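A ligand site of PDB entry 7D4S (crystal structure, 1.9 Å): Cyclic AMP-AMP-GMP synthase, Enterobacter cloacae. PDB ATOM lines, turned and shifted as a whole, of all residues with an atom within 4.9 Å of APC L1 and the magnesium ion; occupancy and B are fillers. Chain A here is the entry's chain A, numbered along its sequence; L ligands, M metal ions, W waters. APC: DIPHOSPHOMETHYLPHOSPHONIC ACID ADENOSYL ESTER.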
ATOM      1  N   GLN A  51       9.824  21.982 -13.723  1.00  0.00           N
ATOM      2  CA  GLN A  51      10.956  22.711 -13.156  1.00  0.00           C
ATOM      3  C   GLN A  51      11.881  21.707 -12.482  1.00  0.00           C
ATOM      4  O   GLN A  51      11.790  20.483 -12.707  1.00  0.00           O
ATOM      5  CB  GLN A  51      10.461  23.798 -12.181  1.00  0.00           C
ATOM      6  CG  GLN A  51       9.685  23.219 -10.972  1.00  0.00           C
ATOM      7  CD  GLN A  51       9.918  24.002  -9.676  1.00  0.00           C
ATOM      8  OE1 GLN A  51      10.626  25.003  -9.663  1.00  0.00           O
ATOM      9  NE2 GLN A  51       9.301  23.554  -8.610  1.00  0.00           N
ATOM     10  N   ASP A  71       9.498  17.948 -10.243  1.00  0.00           N
ATOM     11  CA  ASP A  71       8.989  19.202  -9.707  1.00  0.00           C
ATOM     12  C   ASP A  71       8.133  19.936 -10.732  1.00  0.00           C
ATOM     13  O   ASP A  71       8.534  20.075 -11.902  1.00  0.00           O
ATOM     14  CB  ASP A  71      10.150  20.086  -9.254  1.00  0.00           C
ATOM     15  CG  ASP A  71      10.912  19.455  -8.114  1.00  0.00           C
ATOM     16  OD1 ASP A  71      10.342  19.366  -6.994  1.00  0.00           O
ATOM     17  OD2 ASP A  71      12.049  18.994  -8.357  1.00  0.00           O
ATOM     18  N   ARG A 109       5.373  22.264   2.119  1.00  0.00           N
ATOM     19  CA  ARG A 109       5.196  23.361   1.178  1.00  0.00           C
ATOM     20  C   ARG A 109       4.692  22.898  -0.183  1.00  0.00           C
ATOM     21  O   ARG A 109       4.518  23.760  -1.067  1.00  0.00           O
ATOM     22  CB  ARG A 109       6.498  24.158   1.005  1.00  0.00           C
ATOM     23  CG  ARG A 109       7.622  23.406   0.288  1.00  0.00           C
ATOM     24  CD  ARG A 109       8.256  24.226  -0.843  1.00  0.00           C
ATOM     25  NE  ARG A 109       8.769  25.520  -0.373  1.00  0.00           N
ATOM     26  CZ  ARG A 109       9.977  25.700   0.165  1.00  0.00           C
ATOM     27  NH1 ARG A 109      10.795  24.666   0.315  1.00  0.00           N
ATOM     28  NH2 ARG A 109      10.361  26.898   0.567  1.00  0.00           N
ATOM     29  N   ASP A 121       5.943  16.640  -7.581  1.00  0.00           N
ATOM     30  CA  ASP A 121       6.111  17.528  -6.434  1.00  0.00           C
ATOM     31  C   ASP A 121       5.598  18.897  -6.888  1.00  0.00           C
ATOM     32  O   ASP A 121       6.288  19.622  -7.606  1.00  0.00           O
ATOM     33  CB  ASP A 121       7.585  17.559  -5.990  1.00  0.00           C
ATOM     34  CG  ASP A 121       7.788  18.309  -4.689  1.00  0.00           C
ATOM     35  OD1 ASP A 121       6.782  18.721  -4.082  1.00  0.00           O
ATOM     36  OD2 ASP A 121       8.960  18.496  -4.266  1.00  0.00           O
ATOM     37  N   VAL A 123       4.274  22.653  -6.429  1.00  0.00           N
ATOM     38  CA  VAL A 123       4.311  23.849  -5.580  1.00  0.00           C
ATOM     39  C   VAL A 123       3.370  24.899  -6.172  1.00  0.00           C
ATOM     40  O   VAL A 123       3.348  25.112  -7.392  1.00  0.00           O
ATOM     41  CB  VAL A 123       5.750  24.389  -5.380  1.00  0.00           C
ATOM     42  CG1 VAL A 123       6.370  24.771  -6.715  1.00  0.00           C
ATOM     43  CG2 VAL A 123       5.756  25.574  -4.427  1.00  0.00           C
ATOM     44  N   LEU A 194       6.386  31.551  -3.217  1.00  0.00           N
ATOM     45  CA  LEU A 194       5.979  30.178  -2.910  1.00  0.00           C
ATOM     46  C   LEU A 194       5.888  30.033  -1.390  1.00  0.00           C
ATOM     47  O   LEU A 194       6.384  30.896  -0.665  1.00  0.00           O
ATOM     48  CB  LEU A 194       6.979  29.189  -3.509  1.00  0.00           C
ATOM     49  CG  LEU A 194       8.163  28.770  -2.609  1.00  0.00           C
ATOM     50  CD1 LEU A 194       8.971  27.636  -3.253  1.00  0.00           C
ATOM     51  CD2 LEU A 194       9.062  29.952  -2.309  1.00  0.00           C
ATOM     52  N   PRO A 195       5.290  28.958  -0.861  1.00  0.00           N
ATOM     53  CA  PRO A 195       5.254  28.796   0.599  1.00  0.00           C
ATOM     54  C   PRO A 195       6.636  28.513   1.164  1.00  0.00           C
ATOM     55  O   PRO A 195       7.420  27.753   0.576  1.00  0.00           O
ATOM     56  CB  PRO A 195       4.321  27.579   0.808  1.00  0.00           C
ATOM     57  CG  PRO A 195       3.583  27.402  -0.494  1.00  0.00           C
ATOM     58  CD  PRO A 195       4.525  27.900  -1.553  1.00  0.00           C
ATOM     59  N   ASP A 196       6.939  29.122   2.303  1.00  0.00           N
ATOM     60  CA  ASP A 196       8.146  28.758   3.040  1.00  0.00           C
ATOM     61  C   ASP A 196       8.083  27.289   3.441  1.00  0.00           C
ATOM     62  O   ASP A 196       7.012  26.670   3.458  1.00  0.00           O
ATOM     63  CB  ASP A 196       8.311  29.628   4.279  1.00  0.00           C
ATOM     64  CG  ASP A 196       8.814  31.018   3.942  1.00  0.00           C
ATOM     65  OD1 ASP A 196       9.227  31.238   2.770  1.00  0.00           O
ATOM     66  OD2 ASP A 196       8.776  31.895   4.837  1.00  0.00           O
ATOM     67  N   ARG A 197       9.247  26.713   3.761  1.00  0.00           N
ATOM     68  CA  ARG A 197       9.308  25.262   3.959  1.00  0.00           C
ATOM     69  C   ARG A 197       8.496  24.824   5.166  1.00  0.00           C
ATOM     70  O   ARG A 197       7.818  23.780   5.131  1.00  0.00           O
ATOM     71  CB  ARG A 197      10.764  24.804   4.123  1.00  0.00           C
ATOM     72  CG  ARG A 197      10.913  23.266   4.157  1.00  0.00           C
ATOM     73  CD  ARG A 197      12.282  22.822   4.736  1.00  0.00           C
ATOM     74  NE  ARG A 197      13.391  23.060   3.804  1.00  0.00           N
ATOM     75  CZ  ARG A 197      14.604  22.524   3.942  1.00  0.00           C
ATOM     76  NH1 ARG A 197      15.556  22.794   3.050  1.00  0.00           N
ATOM     77  NH2 ARG A 197      14.862  21.705   4.957  1.00  0.00           N
ATOM     78  N   LYS A 199       6.712  27.223   7.563  1.00  0.00           N
ATOM     79  CA  LYS A 199       5.796  28.180   8.160  1.00  0.00           C
ATOM     80  C   LYS A 199       4.925  28.789   7.069  1.00  0.00           C
ATOM     81  O   LYS A 199       5.259  28.751   5.883  1.00  0.00           O
ATOM     82  CB  LYS A 199       6.546  29.283   8.934  1.00  0.00           C
ATOM     83  CG  LYS A 199       7.515  30.106   8.116  1.00  0.00           C
ATOM     84  CD  LYS A 199       8.426  30.944   9.021  1.00  0.00           C
ATOM     85  CE  LYS A 199       9.443  31.742   8.202  1.00  0.00           C
ATOM     86  NZ  LYS A 199      10.266  32.690   9.047  1.00  0.00           N
ATOM     87  N   ARG A 204      10.451  33.861  -1.703  1.00  0.00           N
ATOM     88  CA  ARG A 204      10.705  34.132  -3.120  1.00  0.00           C
ATOM     89  C   ARG A 204      11.409  32.961  -3.781  1.00  0.00           C
ATOM     90  O   ARG A 204      12.244  32.294  -3.152  1.00  0.00           O
ATOM     91  CB  ARG A 204      11.546  35.395  -3.286  1.00  0.00           C
ATOM     92  CG  ARG A 204      10.712  36.685  -3.108  1.00  0.00           C
ATOM     93  CD  ARG A 204      11.447  37.740  -2.268  1.00  0.00           C
ATOM     94  NE  ARG A 204      12.626  38.261  -2.947  1.00  0.00           N
ATOM     95  CZ  ARG A 204      12.588  39.183  -3.902  1.00  0.00           C
ATOM     96  NH1 ARG A 204      13.713  39.602  -4.466  1.00  0.00           N
ATOM     97  NH2 ARG A 204      11.419  39.692  -4.297  1.00  0.00           N
ATOM     98  N   THR A 205      11.065  32.705  -5.038  1.00  0.00           N
ATOM     99  CA  THR A 205      11.736  31.695  -5.847  1.00  0.00           C
ATOM    100  C   THR A 205      11.696  32.157  -7.299  1.00  0.00           C
ATOM    101  O   THR A 205      10.713  32.760  -7.723  1.00  0.00           O
ATOM    102  CB  THR A 205      11.081  30.314  -5.696  1.00  0.00           C
ATOM    103  OG1 THR A 205      11.854  29.329  -6.388  1.00  0.00           O
ATOM    104  CG2 THR A 205       9.647  30.292  -6.268  1.00  0.00           C
ATOM    105  N   PRO A 207      12.404  30.076 -10.445  1.00  0.00           N
ATOM    106  CA  PRO A 207      12.800  28.872 -11.207  1.00  0.00           C
ATOM    107  C   PRO A 207      13.187  29.171 -12.655  1.00  0.00           C
ATOM    108  O   PRO A 207      14.107  28.530 -13.181  1.00  0.00           O
ATOM    109  CB  PRO A 207      11.556  27.979 -11.149  1.00  0.00           C
ATOM    110  CG  PRO A 207      10.699  28.543 -10.071  1.00  0.00           C
ATOM    111  CD  PRO A 207      11.023  29.994  -9.949  1.00  0.00           C
ATOM    112  N   HIS A 302      19.256  35.472  -1.661  1.00  0.00           N
ATOM    113  CA  HIS A 302      19.155  34.188  -0.975  1.00  0.00           C
ATOM    114  C   HIS A 302      20.496  33.460  -0.976  1.00  0.00           C
ATOM    115  O   HIS A 302      21.137  33.352  -2.031  1.00  0.00           O
ATOM    116  CB  HIS A 302      18.115  33.283  -1.636  1.00  0.00           C
ATOM    117  CG  HIS A 302      16.710  33.623  -1.265  1.00  0.00           C
ATOM    118  ND1 HIS A 302      15.630  32.930  -1.767  1.00  0.00           N
ATOM    119  CD2 HIS A 302      16.203  34.564  -0.430  1.00  0.00           C
ATOM    120  CE1 HIS A 302      14.517  33.428  -1.249  1.00  0.00           C
ATOM    121  NE2 HIS A 302      14.837  34.424  -0.445  1.00  0.00           N
ATOM    122  N   ARG A 307      20.909  26.551   4.844  1.00  0.00           N
ATOM    123  CA  ARG A 307      20.590  25.457   5.765  1.00  0.00           C
ATOM    124  C   ARG A 307      21.733  24.456   5.923  1.00  0.00           C
ATOM    125  O   ARG A 307      21.641  23.545   6.763  1.00  0.00           O
ATOM    126  CB  ARG A 307      19.321  24.734   5.295  1.00  0.00           C
ATOM    127  CG  ARG A 307      18.047  25.546   5.617  1.00  0.00           C
ATOM    128  CD  ARG A 307      16.784  24.675   5.520  1.00  0.00           C
ATOM    129  NE  ARG A 307      15.584  25.414   5.939  1.00  0.00           N
ATOM    130  CZ  ARG A 307      14.740  25.021   6.884  1.00  0.00           C
ATOM    131  NH1 ARG A 307      14.927  23.891   7.540  1.00  0.00           N
ATOM    132  NH2 ARG A 307      13.674  25.771   7.181  1.00  0.00           N
HETATM  133  PG  APC L   1      13.268  29.098   5.995  1.00  0.00           P
HETATM  134  O1G APC L   1      12.503  28.812   7.279  1.00  0.00           O
HETATM  135  O2G APC L   1      14.720  28.570   6.047  1.00  0.00           O
HETATM  136  O3G APC L   1      13.243  30.590   5.733  1.00  0.00           O
HETATM  137  PB  APC L   1      12.903  28.239   3.186  1.00  0.00           P
HETATM  138  O1B APC L   1      11.685  27.732   2.484  1.00  0.00           O
HETATM  139  O2B APC L   1      13.392  29.515   2.568  1.00  0.00           O
HETATM  140  O3B APC L   1      12.455  28.338   4.780  1.00  0.00           O
HETATM  141  PA  APC L   1      14.396  25.961   1.619  1.00  0.00           P
HETATM  142  O1A APC L   1      13.300  24.958   1.699  1.00  0.00           O
HETATM  143  O2A APC L   1      15.712  25.257   1.628  1.00  0.00           O
HETATM  144  C3A APC L   1      14.390  27.091   3.144  1.00  0.00           C
HETATM  145  O5' APC L   1      14.223  26.886   0.286  1.00  0.00           O
HETATM  146  C5' APC L   1      15.197  27.856  -0.057  1.00  0.00           C
HETATM  147  C4' APC L   1      14.755  28.430  -1.452  1.00  0.00           C
HETATM  148  O4' APC L   1      14.787  27.471  -2.359  1.00  0.00           O
HETATM  149  C3' APC L   1      13.269  28.826  -1.395  1.00  0.00           C
HETATM  150  O3' APC L   1      13.156  30.100  -0.942  1.00  0.00           O
HETATM  151  C2' APC L   1      12.876  28.712  -2.858  1.00  0.00           C
HETATM  152  O2' APC L   1      13.410  29.919  -3.545  1.00  0.00           O
HETATM  153  C1' APC L   1      13.549  27.669  -3.319  1.00  0.00           C
HETATM  154  N9  APC L   1      12.787  26.451  -3.331  1.00  0.00           N
HETATM  155  C8  APC L   1      12.812  25.481  -2.401  1.00  0.00           C
HETATM  156  N7  APC L   1      11.976  24.512  -2.790  1.00  0.00           N
HETATM  157  C5  APC L   1      11.438  24.888  -3.973  1.00  0.00           C
HETATM  158  C6  APC L   1      10.532  24.290  -4.824  1.00  0.00           C
HETATM  159  N6  APC L   1       9.828  23.008  -4.692  1.00  0.00           N
HETATM  160  N1  APC L   1      10.167  24.886  -5.966  1.00  0.00           N
HETATM  161  C2  APC L   1      10.670  26.080  -6.290  1.00  0.00           C
HETATM  162  N3  APC L   1      11.568  26.678  -5.450  1.00  0.00           N
HETATM  163  C4  APC L   1      11.946  26.081  -4.309  1.00  0.00           C
HETATM  164  PG  APC L   2      16.325  16.208  -6.951  1.00  0.00           P
HETATM  165  O1G APC L   2      17.082  15.596  -5.799  1.00  0.00           O
HETATM  166  O2G APC L   2      14.833  16.419  -6.591  1.00  0.00           O
HETATM  167  O3G APC L   2      16.514  15.435  -8.251  1.00  0.00           O
HETATM  168  PB  APC L   2      16.249  19.094  -7.150  1.00  0.00           P
HETATM  169  O1B APC L   2      17.127  20.206  -7.628  1.00  0.00           O
HETATM  170  O2B APC L   2      14.950  19.021  -7.924  1.00  0.00           O
HETATM  171  O3B APC L   2      17.049  17.665  -7.263  1.00  0.00           O
HETATM  172  PA  APC L   2      14.204  19.679  -4.907  1.00  0.00           P
HETATM  173  O1A APC L   2      14.065  19.550  -3.430  1.00  0.00           O
HETATM  174  O2A APC L   2      13.222  18.790  -5.630  1.00  0.00           O
HETATM  175  C3A APC L   2      16.009  19.245  -5.298  1.00  0.00           C
HETATM  176  O5' APC L   2      13.996  21.221  -5.333  1.00  0.00           O
HETATM  177  C5' APC L   2      13.216  21.559  -6.444  1.00  0.00           C
HETATM  178  C4' APC L   2      13.775  22.912  -6.993  1.00  0.00           C
HETATM  179  O4' APC L   2      13.564  23.867  -6.091  1.00  0.00           O
HETATM  180  C3' APC L   2      15.310  22.833  -7.130  1.00  0.00           C
HETATM  181  O3' APC L   2      15.684  22.223  -8.281  1.00  0.00           O
HETATM  182  C2' APC L   2      15.614  24.340  -7.074  1.00  0.00           C
HETATM  183  O2' APC L   2      15.265  24.896  -8.407  1.00  0.00           O
HETATM  184  C1' APC L   2      14.823  24.819  -6.108  1.00  0.00           C
HETATM  185  N9  APC L   2      15.534  24.757  -4.869  1.00  0.00           N
HETATM  186  C8  APC L   2      15.547  23.758  -3.965  1.00  0.00           C
HETATM  187  N7  APC L   2      16.385  24.076  -2.984  1.00  0.00           N
HETATM  188  C5  APC L   2      16.925  25.275  -3.292  1.00  0.00           C
HETATM  189  C6  APC L   2      17.845  26.064  -2.633  1.00  0.00           C
HETATM  190  N6  APC L   2      18.536  25.825  -1.366  1.00  0.00           N
HETATM  191  N1  APC L   2      18.233  27.234  -3.163  1.00  0.00           N
HETATM  192  C2  APC L   2      17.708  27.657  -4.321  1.00  0.00           C
HETATM  193  N3  APC L   2      16.787  26.862  -4.987  1.00  0.00           N
HETATM  194  C4  APC L   2      16.422  25.691  -4.448  1.00  0.00           C
HETATM  195 MG    MG M   1      14.407  30.832   3.964  1.00  0.00          MG
HETATM  196  O   HOH W   1      18.027  26.757   2.204  1.00  0.00           O
HETATM  197  O   HOH W   2       9.016  21.083  -2.605  1.00  0.00           O
HETATM  198  O   HOH W   3      10.853  27.986   9.748  1.00  0.00           O
HETATM  199  O   HOH W   4      12.449  21.824  -1.928  1.00  0.00           O
HETATM  200  O   HOH W   5       8.447  21.337  -6.619  1.00  0.00           O
HETATM  201  O   HOH W   6      15.033  31.587   1.509  1.00  0.00           O
HETATM  202  O   HOH W   7      10.721  29.731   0.811  1.00  0.00           O
HETATM  203  O   HOH W   8      17.061  28.883   4.574  1.00  0.00           O
HETATM  204  O   HOH W   9      17.614  23.408   0.397  1.00  0.00           O
HETATM  205  O   HOH W  10      10.156  27.757   6.780  1.00  0.00           O
HETATM  206  O   HOH W  11      16.196  31.000  -3.618  1.00  0.00           O
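The backbone carbonyl oxygen (O) of Arg 204 sits at hydrogen-bond distance from an oxygen (O2') of APC L1 (2.7 Å).
O1B of APC L1 sits at hydrogen-bond distance from N of Arg 197.
The guanidinium group (NH2) of Arg 109 lies within salt-bridge range of an oxygen (O1B) of APC L1.
A nitrogen (N3) of APC L1 is in hydrogen-bond range of the side-chain hydroxyl (OG1) of Thr 205 (2.8 Å).
N1 of APC L1 lies within hydrogen-bond range of NE2 of Gln 51 (3.1 Å).
NE of Arg 197 is in salt-bridge range of O1A of APC L1.
The guanidinium group of Arg 307 lies within salt-bridge range of an oxygen (O2G) of APC L1 (3.2 Å).
The backbone NH of Gln 51 sits at hydrogen-bond distance from the backbone carbonyl oxygen of Asp 71, at 2.9 Å.
NE of Arg 109 sits at hydrogen-bond distance from O of Pro 195.
Val 123 touches APC L1.
Leu 194 touches APC L1 (CD1 to C4, 3.5 Å).
Asp 196 touches APC L1.
His 302 touches APC L1.
Hydrophobic or aromatic side chains that line APC L1: Val 123, Leu 194 and His 302.
Ten residues have an atom within 4 Å of APC L1: Gln 51, Arg 109, Val 123, Leu 194, Asp 196, Arg 197, Arg 204, Thr 205, His 302 and Arg 307.
Along chain A the residues within 4 Å of APC L1 span positions 51 to 307.
The nearest printed residue that does not touch APC L1 is Lys 199 (4.3 Å).
No residue comes within 4 Å of the magnesium ion.
The magnesium ion is bound by an oxygen (O3G) of APC L1 (2.1 Å) and an oxygen (O2B) of APC L1 (2.2 Å).
Slightly farther from the magnesium ion lies water W6 (2.6 Å).
Water W6 bridges an oxygen (O3') of APC L1 and a ring nitrogen (NE2) of His 302.
Water W10 bridges O1G of APC L1 (2.6 Å) and N of Arg 197 (3.3 Å).
Water W7 lies within hydrogen-bond range of O1B of APC L1 (2.8 Å), NH2 of Arg 109 (2.9 Å) and OD1 of Asp 196 (2.9 Å).
Water W5 lies within hydrogen-bond range of N6 of APC L1 (2.9 Å), O of Asp 121 (2.9 Å) and NE2 of Gln 51 (3.1 Å).
Water W9 lies within hydrogen-bond range of O2A of APC L1 (2.9 Å), N6 of APC L2 (3.1 Å) and NH1 of Arg 197 (3.4 Å).
Water W11 bridges a ring nitrogen (ND1) of His 302 (2.7 Å) and an oxygen (O2') of APC L1 (3.0 Å).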
